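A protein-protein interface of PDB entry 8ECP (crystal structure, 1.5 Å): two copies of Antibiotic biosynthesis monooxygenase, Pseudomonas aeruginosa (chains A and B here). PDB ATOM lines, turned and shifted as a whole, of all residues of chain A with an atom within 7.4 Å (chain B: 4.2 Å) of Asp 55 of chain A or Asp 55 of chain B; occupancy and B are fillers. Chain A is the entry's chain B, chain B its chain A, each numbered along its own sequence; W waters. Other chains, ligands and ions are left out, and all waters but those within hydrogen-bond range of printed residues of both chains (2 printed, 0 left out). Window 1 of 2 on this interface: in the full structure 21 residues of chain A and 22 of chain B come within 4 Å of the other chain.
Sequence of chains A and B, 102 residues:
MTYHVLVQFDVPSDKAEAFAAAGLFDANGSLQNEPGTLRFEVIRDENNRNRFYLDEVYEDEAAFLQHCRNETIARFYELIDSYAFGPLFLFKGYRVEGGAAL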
ATOM      1  N   HIS A   4      14.334  11.357  18.208  1.00  0.00           N
ATOM      2  CA  HIS A   4      14.188  10.026  17.644  1.00  0.00           C
ATOM      3  C   HIS A   4      15.214   9.081  18.247  1.00  0.00           C
ATOM      4  O   HIS A   4      16.407   9.404  18.308  1.00  0.00           O
ATOM      5  CB  HIS A   4      14.305  10.083  16.122  1.00  0.00           C
ATOM      6  CG  HIS A   4      13.288  10.974  15.482  1.00  0.00           C
ATOM      7  ND1 HIS A   4      12.375  10.503  14.564  1.00  0.00           N
ATOM      8  CD2 HIS A   4      13.001  12.287  15.660  1.00  0.00           C
ATOM      9  CE1 HIS A   4      11.581  11.491  14.192  1.00  0.00           C
ATOM     10  NE2 HIS A   4      11.942  12.585  14.835  1.00  0.00           N
ATOM     11  N   VAL A   5      14.741   7.914  18.677  1.00  0.00           N
ATOM     12  CA  VAL A   5      15.538   6.917  19.376  1.00  0.00           C
ATOM     13  C   VAL A   5      15.316   5.576  18.694  1.00  0.00           C
ATOM     14  O   VAL A   5      14.187   5.071  18.665  1.00  0.00           O
ATOM     15  CB  VAL A   5      15.176   6.833  20.871  1.00  0.00           C
ATOM     16  CG1 VAL A   5      16.095   5.855  21.582  1.00  0.00           C
ATOM     17  CG2 VAL A   5      15.291   8.210  21.534  1.00  0.00           C
ATOM     18  N   LEU A   6      16.376   5.013  18.126  1.00  0.00           N
ATOM     19  CA  LEU A   6      16.337   3.702  17.496  1.00  0.00           C
ATOM     20  C   LEU A   6      17.053   2.686  18.379  1.00  0.00           C
ATOM     21  O   LEU A   6      18.238   2.849  18.668  1.00  0.00           O
ATOM     22  CB  LEU A   6      17.015   3.754  16.136  1.00  0.00           C
ATOM     23  CG  LEU A   6      16.689   2.481  15.369  1.00  0.00           C
ATOM     24  CD1 LEU A   6      15.242   2.480  14.852  1.00  0.00           C
ATOM     25  CD2 LEU A   6      17.654   2.358  14.281  1.00  0.00           C
ATOM     26  N   VAL A   7      16.334   1.642  18.764  1.00  0.00           N
ATOM     27  CA  VAL A   7      16.801   0.622  19.687  1.00  0.00           C
ATOM     28  C   VAL A   7      16.817  -0.703  18.943  1.00  0.00           C
ATOM     29  O   VAL A   7      15.910  -0.995  18.153  1.00  0.00           O
ATOM     30  CB  VAL A   7      15.833   0.539  20.887  1.00  0.00           C
ATOM     31  CG1 VAL A   7      16.441  -0.285  21.980  1.00  0.00           C
ATOM     32  CG2 VAL A   7      15.457   1.944  21.408  1.00  0.00           C
ATOM     33  N   ARG A  39       5.352   8.464  18.685  1.00  0.00           N
ATOM     34  CA  ARG A  39       5.309   7.390  17.708  1.00  0.00           C
ATOM     35  C   ARG A  39       6.177   6.279  18.269  1.00  0.00           C
ATOM     36  O   ARG A  39       7.161   6.549  18.959  1.00  0.00           O
ATOM     37  CB  ARG A  39       5.846   7.869  16.353  1.00  0.00           C
ATOM     38  CG  ARG A  39       5.364   7.083  15.139  1.00  0.00           C
ATOM     39  CD  ARG A  39       5.875   7.696  13.838  1.00  0.00           C
ATOM     40  NE  ARG A  39       7.315   7.498  13.675  1.00  0.00           N
ATOM     41  CZ  ARG A  39       8.122   8.334  13.038  1.00  0.00           C
ATOM     42  NH1 ARG A  39       7.675   9.459  12.500  1.00  0.00           N
ATOM     43  NH2 ARG A  39       9.415   8.040  12.946  1.00  0.00           N
ATOM     44  N   PHE A  40       5.803   5.034  17.996  1.00  0.00           N
ATOM     45  CA  PHE A  40       6.512   3.906  18.595  1.00  0.00           C
ATOM     46  C   PHE A  40       6.212   2.682  17.744  1.00  0.00           C
ATOM     47  O   PHE A  40       5.096   2.155  17.784  1.00  0.00           O
ATOM     48  CB  PHE A  40       6.055   3.727  20.041  1.00  0.00           C
ATOM     49  CG  PHE A  40       7.048   3.021  20.928  1.00  0.00           C
ATOM     50  CD1 PHE A  40       7.374   1.697  20.723  1.00  0.00           C
ATOM     51  CD2 PHE A  40       7.680   3.712  21.961  1.00  0.00           C
ATOM     52  CE1 PHE A  40       8.265   1.049  21.552  1.00  0.00           C
ATOM     53  CE2 PHE A  40       8.593   3.073  22.786  1.00  0.00           C
ATOM     54  CZ  PHE A  40       8.886   1.738  22.579  1.00  0.00           C
ATOM     55  N   GLU A  41       7.195   2.256  16.957  1.00  0.00           N
ATOM     56  CA  GLU A  41       7.022   1.171  16.004  1.00  0.00           C
ATOM     57  C   GLU A  41       7.982   0.038  16.327  1.00  0.00           C
ATOM     58  O   GLU A  41       9.118   0.270  16.753  1.00  0.00           O
ATOM     59  CB  GLU A  41       7.272   1.647  14.565  1.00  0.00           C
ATOM     60  CG  GLU A  41       6.194   2.581  14.055  1.00  0.00           C
ATOM     61  CD  GLU A  41       6.565   3.290  12.762  1.00  0.00           C
ATOM     62  OE1 GLU A  41       7.768   3.503  12.485  1.00  0.00           O
ATOM     63  OE2 GLU A  41       5.629   3.621  12.013  1.00  0.00           O
ATOM     64  N   VAL A  42       7.509  -1.184  16.114  1.00  0.00           N
ATOM     65  CA  VAL A  42       8.299  -2.400  16.258  1.00  0.00           C
ATOM     66  C   VAL A  42       8.570  -2.927  14.859  1.00  0.00           C
ATOM     67  O   VAL A  42       7.626  -3.148  14.095  1.00  0.00           O
ATOM     68  CB  VAL A  42       7.531  -3.450  17.080  1.00  0.00           C
ATOM     69  CG1 VAL A  42       8.378  -4.698  17.265  1.00  0.00           C
ATOM     70  CG2 VAL A  42       7.062  -2.858  18.425  1.00  0.00           C
ATOM     71  N   ILE A  43       9.844  -3.139  14.525  1.00  0.00           N
ATOM     72  CA  ILE A  43      10.249  -3.530  13.176  1.00  0.00           C
ATOM     73  C   ILE A  43      11.055  -4.821  13.267  1.00  0.00           C
ATOM     74  O   ILE A  43      12.002  -4.907  14.055  1.00  0.00           O
ATOM     75  CB  ILE A  43      11.069  -2.415  12.492  1.00  0.00           C
ATOM     76  CG1 ILE A  43      10.246  -1.136  12.328  1.00  0.00           C
ATOM     77  CG2 ILE A  43      11.588  -2.860  11.137  1.00  0.00           C
ATOM     78  CD1 ILE A  43      11.099   0.114  12.218  1.00  0.00           C
ATOM     79  N   TYR A  53      13.897  -3.968  15.890  1.00  0.00           N
ATOM     80  CA  TYR A  53      14.213  -2.566  16.127  1.00  0.00           C
ATOM     81  C   TYR A  53      12.970  -1.870  16.642  1.00  0.00           C
ATOM     82  O   TYR A  53      11.864  -2.140  16.176  1.00  0.00           O
ATOM     83  CB  TYR A  53      14.667  -1.897  14.811  1.00  0.00           C
ATOM     84  CG  TYR A  53      15.671  -2.728  14.058  1.00  0.00           C
ATOM     85  CD1 TYR A  53      17.027  -2.667  14.378  1.00  0.00           C
ATOM     86  CD2 TYR A  53      15.273  -3.603  13.054  1.00  0.00           C
ATOM     87  CE1 TYR A  53      17.961  -3.437  13.697  1.00  0.00           C
ATOM     88  CE2 TYR A  53      16.198  -4.388  12.379  1.00  0.00           C
ATOM     89  CZ  TYR A  53      17.540  -4.297  12.710  1.00  0.00           C
ATOM     90  OH  TYR A  53      18.465  -5.063  12.031  1.00  0.00           O
ATOM     91  N   LEU A  54      13.153  -0.988  17.619  1.00  0.00           N
ATOM     92  CA  LEU A  54      12.093  -0.107  18.083  1.00  0.00           C
ATOM     93  C   LEU A  54      12.438   1.292  17.593  1.00  0.00           C
ATOM     94  O   LEU A  54      13.532   1.804  17.875  1.00  0.00           O
ATOM     95  CB  LEU A  54      11.988  -0.131  19.608  1.00  0.00           C
ATOM     96  CG  LEU A  54      11.868  -1.500  20.282  1.00  0.00           C
ATOM     97  CD1 LEU A  54      11.690  -1.340  21.807  1.00  0.00           C
ATOM     98  CD2 LEU A  54      10.740  -2.312  19.685  1.00  0.00           C
ATOM     99  N   ASP A  55      11.534   1.886  16.831  1.00  0.00           N
ATOM    100  CA  ASP A  55      11.690   3.229  16.278  1.00  0.00           C
ATOM    101  C   ASP A  55      10.763   4.141  17.070  1.00  0.00           C
ATOM    102  O   ASP A  55       9.539   4.123  16.886  1.00  0.00           O
ATOM    103  CB  ASP A  55      11.359   3.225  14.790  1.00  0.00           C
ATOM    104  CG  ASP A  55      11.821   4.480  14.076  1.00  0.00           C
ATOM    105  OD1 ASP A  55      12.189   5.483  14.741  1.00  0.00           O
ATOM    106  OD2 ASP A  55      11.827   4.444  12.833  1.00  0.00           O
ATOM    107  N   GLU A  56      11.354   4.938  17.950  1.00  0.00           N
ATOM    108  CA  GLU A  56      10.621   5.712  18.943  1.00  0.00           C
ATOM    109  C   GLU A  56      10.791   7.207  18.707  1.00  0.00           C
ATOM    110  O   GLU A  56      11.896   7.677  18.412  1.00  0.00           O
ATOM    111  CB  GLU A  56      11.090   5.359  20.360  1.00  0.00           C
ATOM    112  CG  GLU A  56      11.382   3.872  20.584  1.00  0.00           C
ATOM    113  CD  GLU A  56      11.904   3.581  21.980  1.00  0.00           C
ATOM    114  OE1 GLU A  56      12.170   4.539  22.734  1.00  0.00           O
ATOM    115  OE2 GLU A  56      12.083   2.390  22.312  1.00  0.00           O
ATOM    116  N   VAL A  57       9.700   7.962  18.850  1.00  0.00           N
ATOM    117  CA  VAL A  57       9.728   9.410  18.657  1.00  0.00           C
ATOM    118  C   VAL A  57       9.104  10.099  19.868  1.00  0.00           C
ATOM    119  O   VAL A  57       7.987   9.746  20.284  1.00  0.00           O
ATOM    120  CB  VAL A  57       9.010   9.839  17.360  1.00  0.00           C
ATOM    121  CG1 VAL A  57       9.097  11.345  17.187  1.00  0.00           C
ATOM    122  CG2 VAL A  57       9.577   9.104  16.138  1.00  0.00           C
ATOM    123  N   TYR A  58       9.806  11.112  20.394  1.00  0.00           N
ATOM    124  CA  TYR A  58       9.422  11.863  21.586  1.00  0.00           C
ATOM    125  C   TYR A  58       9.428  13.355  21.279  1.00  0.00           C
ATOM    126  O   TYR A  58      10.067  13.810  20.330  1.00  0.00           O
ATOM    127  CB  TYR A  58      10.380  11.569  22.752  1.00  0.00           C
ATOM    128  CG  TYR A  58      10.405  10.105  23.086  1.00  0.00           C
ATOM    129  CD1 TYR A  58       9.456   9.557  23.942  1.00  0.00           C
ATOM    130  CD2 TYR A  58      11.335   9.250  22.491  1.00  0.00           C
ATOM    131  CE1 TYR A  58       9.448   8.208  24.233  1.00  0.00           C
ATOM    132  CE2 TYR A  58      11.332   7.898  22.770  1.00  0.00           C
ATOM    133  CZ  TYR A  58      10.384   7.383  23.641  1.00  0.00           C
ATOM    134  OH  TYR A  58      10.354   6.043  23.927  1.00  0.00           O
ATOM    135  N   PHE A  91      20.938   4.836  17.459  1.00  0.00           N
ATOM    136  CA  PHE A  91      21.175   6.272  17.516  1.00  0.00           C
ATOM    137  C   PHE A  91      20.119   6.951  18.367  1.00  0.00           C
ATOM    138  O   PHE A  91      19.035   6.412  18.611  1.00  0.00           O
ATOM    139  CB  PHE A  91      21.269   6.930  16.134  1.00  0.00           C
ATOM    140  CG  PHE A  91      19.981   6.983  15.374  1.00  0.00           C
ATOM    141  CD1 PHE A  91      19.000   7.925  15.659  1.00  0.00           C
ATOM    142  CD2 PHE A  91      19.788   6.137  14.303  1.00  0.00           C
ATOM    143  CE1 PHE A  91      17.824   7.965  14.923  1.00  0.00           C
ATOM    144  CE2 PHE A  91      18.646   6.189  13.561  1.00  0.00           C
ATOM    145  CZ  PHE A  91      17.655   7.105  13.864  1.00  0.00           C
ATOM    146  N   VAL B   5      13.398   1.292   5.994  1.00  0.00           N
ATOM    147  CA  VAL B   5      14.809   1.303   5.626  1.00  0.00           C
ATOM    148  C   VAL B   5      15.495   2.427   6.383  1.00  0.00           C
ATOM    149  O   VAL B   5      15.065   3.584   6.310  1.00  0.00           O
ATOM    150  CB  VAL B   5      14.979   1.483   4.100  1.00  0.00           C
ATOM    151  CG1 VAL B   5      16.446   1.586   3.715  1.00  0.00           C
ATOM    152  CG2 VAL B   5      14.303   0.347   3.353  1.00  0.00           C
ATOM    153  N   LEU B   6      16.570   2.101   7.089  1.00  0.00           N
ATOM    154  CA  LEU B   6      17.338   3.090   7.842  1.00  0.00           C
ATOM    155  C   LEU B   6      18.726   3.219   7.230  1.00  0.00           C
ATOM    156  O   LEU B   6      19.465   2.233   7.164  1.00  0.00           O
ATOM    157  CB  LEU B   6      17.459   2.664   9.293  1.00  0.00           C
ATOM    158  CG  LEU B   6      18.031   3.827  10.098  1.00  0.00           C
ATOM    159  CD1 LEU B   6      17.076   5.012  10.251  1.00  0.00           C
ATOM    160  CD2 LEU B   6      18.542   3.341  11.377  1.00  0.00           C
ATOM    161  N   ARG B  39       6.760   7.703   4.268  1.00  0.00           N
ATOM    162  CA  ARG B  39       7.369   8.555   5.277  1.00  0.00           C
ATOM    163  C   ARG B  39       8.851   8.646   4.969  1.00  0.00           C
ATOM    164  O   ARG B  39       9.449   7.681   4.489  1.00  0.00           O
ATOM    165  CB  ARG B  39       7.144   7.987   6.680  1.00  0.00           C
ATOM    166  CG  ARG B  39       7.154   9.011   7.807  1.00  0.00           C
ATOM    167  CD  ARG B  39       6.707   8.355   9.095  1.00  0.00           C
ATOM    168  NE  ARG B  39       7.732   7.448   9.600  1.00  0.00           N
ATOM    169  CZ  ARG B  39       7.485   6.382  10.349  1.00  0.00           C
ATOM    170  NH1 ARG B  39       6.250   6.022  10.655  1.00  0.00           N
ATOM    171  NH2 ARG B  39       8.504   5.656  10.798  1.00  0.00           N
ATOM    172  N   PHE B  40       9.451   9.806   5.249  1.00  0.00           N
ATOM    173  CA  PHE B  40      10.858  10.010   4.902  1.00  0.00           C
ATOM    174  C   PHE B  40      11.400  11.129   5.790  1.00  0.00           C
ATOM    175  O   PHE B  40      11.107  12.306   5.550  1.00  0.00           O
ATOM    176  CB  PHE B  40      10.986  10.353   3.426  1.00  0.00           C
ATOM    177  CG  PHE B  40      12.343  10.053   2.838  1.00  0.00           C
ATOM    178  CD1 PHE B  40      13.467  10.717   3.281  1.00  0.00           C
ATOM    179  CD2 PHE B  40      12.483   9.112   1.833  1.00  0.00           C
ATOM    180  CE1 PHE B  40      14.703  10.465   2.725  1.00  0.00           C
ATOM    181  CE2 PHE B  40      13.714   8.852   1.272  1.00  0.00           C
ATOM    182  CZ  PHE B  40      14.831   9.528   1.729  1.00  0.00           C
ATOM    183  N   GLU B  41      12.214  10.759   6.776  1.00  0.00           N
ATOM    184  CA  GLU B  41      12.720  11.689   7.774  1.00  0.00           C
ATOM    185  C   GLU B  41      14.240  11.741   7.738  1.00  0.00           C
ATOM    186  O   GLU B  41      14.905  10.706   7.632  1.00  0.00           O
ATOM    187  CB  GLU B  41      12.233  11.308   9.180  1.00  0.00           C
ATOM    188  CG  GLU B  41      10.722  11.501   9.367  1.00  0.00           C
ATOM    189  CD  GLU B  41      10.176  10.854  10.633  1.00  0.00           C
ATOM    190  OE1 GLU B  41      10.785   9.892  11.142  1.00  0.00           O
ATOM    191  OE2 GLU B  41       9.130  11.324  11.126  1.00  0.00           O
ATOM    192  N   ILE B  43      17.384  12.746  10.050  1.00  0.00           N
ATOM    193  CA  ILE B  43      17.674  12.859  11.476  1.00  0.00           C
ATOM    194  C   ILE B  43      19.166  13.109  11.630  1.00  0.00           C
ATOM    195  O   ILE B  43      19.973  12.438  10.988  1.00  0.00           O
ATOM    196  CB  ILE B  43      17.275  11.570  12.221  1.00  0.00           C
ATOM    197  CG1 ILE B  43      15.783  11.285  12.021  1.00  0.00           C
ATOM    198  CG2 ILE B  43      17.643  11.665  13.711  1.00  0.00           C
ATOM    199  CD1 ILE B  43      15.383   9.848  12.326  1.00  0.00           C
ATOM    200  N   TYR B  53      20.982  10.304   9.554  1.00  0.00           N
ATOM    201  CA  TYR B  53      20.211   9.100   9.277  1.00  0.00           C
ATOM    202  C   TYR B  53      18.993   9.463   8.447  1.00  0.00           C
ATOM    203  O   TYR B  53      18.377  10.518   8.651  1.00  0.00           O
ATOM    204  CB  TYR B  53      19.772   8.406  10.563  1.00  0.00           C
ATOM    205  CG  TYR B  53      20.877   8.305  11.591  1.00  0.00           C
ATOM    206  CD1 TYR B  53      21.834   7.290  11.527  1.00  0.00           C
ATOM    207  CD2 TYR B  53      20.974   9.240  12.617  1.00  0.00           C
ATOM    208  CE1 TYR B  53      22.861   7.208  12.484  1.00  0.00           C
ATOM    209  CE2 TYR B  53      22.001   9.168  13.573  1.00  0.00           C
ATOM    210  CZ  TYR B  53      22.934   8.149  13.500  1.00  0.00           C
ATOM    211  OH  TYR B  53      23.933   8.084  14.451  1.00  0.00           O
ATOM    212  N   LEU B  54      18.671   8.602   7.490  1.00  0.00           N
ATOM    213  CA  LEU B  54      17.426   8.700   6.737  1.00  0.00           C
ATOM    214  C   LEU B  54      16.548   7.540   7.170  1.00  0.00           C
ATOM    215  O   LEU B  54      16.942   6.378   7.045  1.00  0.00           O
ATOM    216  CB  LEU B  54      17.693   8.635   5.233  1.00  0.00           C
ATOM    217  CG  LEU B  54      18.722   9.610   4.671  1.00  0.00           C
ATOM    218  CD1 LEU B  54      18.778   9.449   3.177  1.00  0.00           C
ATOM    219  CD2 LEU B  54      18.333  11.050   5.035  1.00  0.00           C
ATOM    220  N   ASP B  55      15.379   7.856   7.706  1.00  0.00           N
ATOM    221  CA  ASP B  55      14.394   6.883   8.171  1.00  0.00           C
ATOM    222  C   ASP B  55      13.256   6.885   7.163  1.00  0.00           C
ATOM    223  O   ASP B  55      12.452   7.821   7.120  1.00  0.00           O
ATOM    224  CB  ASP B  55      13.915   7.262   9.567  1.00  0.00           C
ATOM    225  CG  ASP B  55      13.164   6.139  10.248  1.00  0.00           C
ATOM    226  OD1 ASP B  55      12.773   5.169   9.564  1.00  0.00           O
ATOM    227  OD2 ASP B  55      12.951   6.238  11.470  1.00  0.00           O
ATOM    228  N   GLU B  56      13.220   5.847   6.338  1.00  0.00           N
ATOM    229  CA  GLU B  56      12.351   5.771   5.179  1.00  0.00           C
ATOM    230  C   GLU B  56      11.322   4.662   5.359  1.00  0.00           C
ATOM    231  O   GLU B  56      11.643   3.565   5.824  1.00  0.00           O
ATOM    232  CB  GLU B  56      13.195   5.503   3.930  1.00  0.00           C
ATOM    233  CG  GLU B  56      14.473   6.330   3.889  1.00  0.00           C
ATOM    234  CD  GLU B  56      15.347   5.996   2.692  1.00  0.00           C
ATOM    235  OE1 GLU B  56      15.007   5.046   1.960  1.00  0.00           O
ATOM    236  OE2 GLU B  56      16.369   6.692   2.487  1.00  0.00           O
HETATM  237  O   HOH W   1      11.107   3.311  10.625  1.00  0.00           O
HETATM  238  O   HOH W   2      12.559   7.831  13.759  1.00  0.00           O
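The guanidinium group (NH1) of Arg 39 of chain B lies within salt-bridge range of the side-chain carboxylate (OE2) of Glu 41 of chain A (2.8 Å). The side-chain carboxylate (OE2) of Glu 41 of chain B is in salt-bridge range of the guanidinium group (NH1) of Arg 39 of chain A, at 2.7 Å. OD2 of Asp 55 of chain A lies close to OD2 of Asp 55 of chain B, at 2.5 Å. The guanidinium group of Arg 39 of chain A sits close to the guanidinium group of Arg 39 of chain B (3.3 Å).
N of Asp 55 of chain B sits at hydrogen-bond distance from O of Glu 41 of chain B (2.9 Å). The backbone carbonyl oxygen (O) of Ile 43 of chain B lies within hydrogen-bond range of the backbone NH (N) of Tyr 53 of chain B (2.8 Å). The backbone NH (N) of Leu 6 of chain A lies within hydrogen-bond range of the backbone carbonyl oxygen (O) of Phe 91 of chain A (3.0 Å). The backbone carbonyl oxygen (O) of Arg 39 of chain A lies within hydrogen-bond range of the backbone NH (N) of Val 57 of chain A (2.9 Å). The backbone carbonyl oxygen of Glu 41 of chain A is in hydrogen-bond range of the backbone NH of Asp 55 of chain A (2.9 Å).
CE1 of His 4 of chain A touches OE1 of Glu 41 of chain B, 3.5 Å away. His 4 of chain A touches Ile 43 of chain B. Leu 6 of chain A touches Leu 6 of chain B. Phe 91 of chain A touches Leu 6 of chain B. Ile 43 of chain B touches Phe 91 of chain A (CD1 to CZ, 3.9 Å). Phe 91 of chain A touches Tyr 53 of chain B.
Tyr 53 of chain A touches none of the printed residues of chain B. Of chain B, only Asp 55 (2.5 Å) comes within 4 Å of Asp 55 of chain A. Of the printed residues of chain B, Phe 91 of chain A touches Leu 6 (3.6 Å), Ile 43 (3.9 Å) and Tyr 53 (3.3 Å). Of the printed residues of chain A, Arg 39 of chain B touches Arg 39 (3.3 Å) and Glu 41 (2.8 Å). Asp 55 of chain B touches just one residue of chain A: Asp 55 (2.5 Å). The nearest residue of chain B that does not touch Asp 55 of chain A is Arg 39 of chain B (4.1 Å).
Of the 16 printed residues of chain A, 6 touch a printed residue of chain B. Hydrophobic or aromatic side chains of chain A within 4 Å of the printed part of chain B: His 4, Leu 6 and Phe 91. Of the 10 printed residues of chain B, 6 touch a printed residue of chain A. Hydrophobic or aromatic side chains of chain B within 4 Å of the printed part of chain A: Leu 6, Ile 43 and Tyr 53. Among the printed residues, 10 pairs touch across the chains. Among the printed residues, Asp or Glu carboxylates within 4 Å of a Lys or Arg side-chain nitrogen of the other chain: Arg 39 of chain A with Glu 41 of chain B (2.7 Å) and Glu 41 of chain A with Arg 39 of chain B (2.8 Å).
Leu 6 of chain B touches its own counterpart, Leu 6 of chain A. Arg 39 of chain A touches its own counterpart, Arg 39 of chain B. Arg 39 of chain A touches Glu 41 of chain B, and with the chains exchanged Glu 41 of chain A touches Arg 39 of chain B. Asp 55 of chain B touches its own counterpart, Asp 55 of chain A. Positions printed for both chains: 5, 6, 39, 40, 41, 43, 53, 54, 55 and 56. Of the 10 pairs that touch across the chains among the printed residues, 5 have their exchanged pair printed and touching as well.
Water W2 lies within hydrogen-bond range of the side-chain carboxylate (OD1) of Asp 55 of chain A, a ring nitrogen (ND1) of His 4 of chain A, the side-chain carboxylate (OD2) of Asp 55 of chain B and the guanidinium group (NH2) of Arg 39 of chain A. Water W1 lies within hydrogen-bond range of OD2 of Asp 55 of chain A and OD1 of Asp 55 of chain B.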
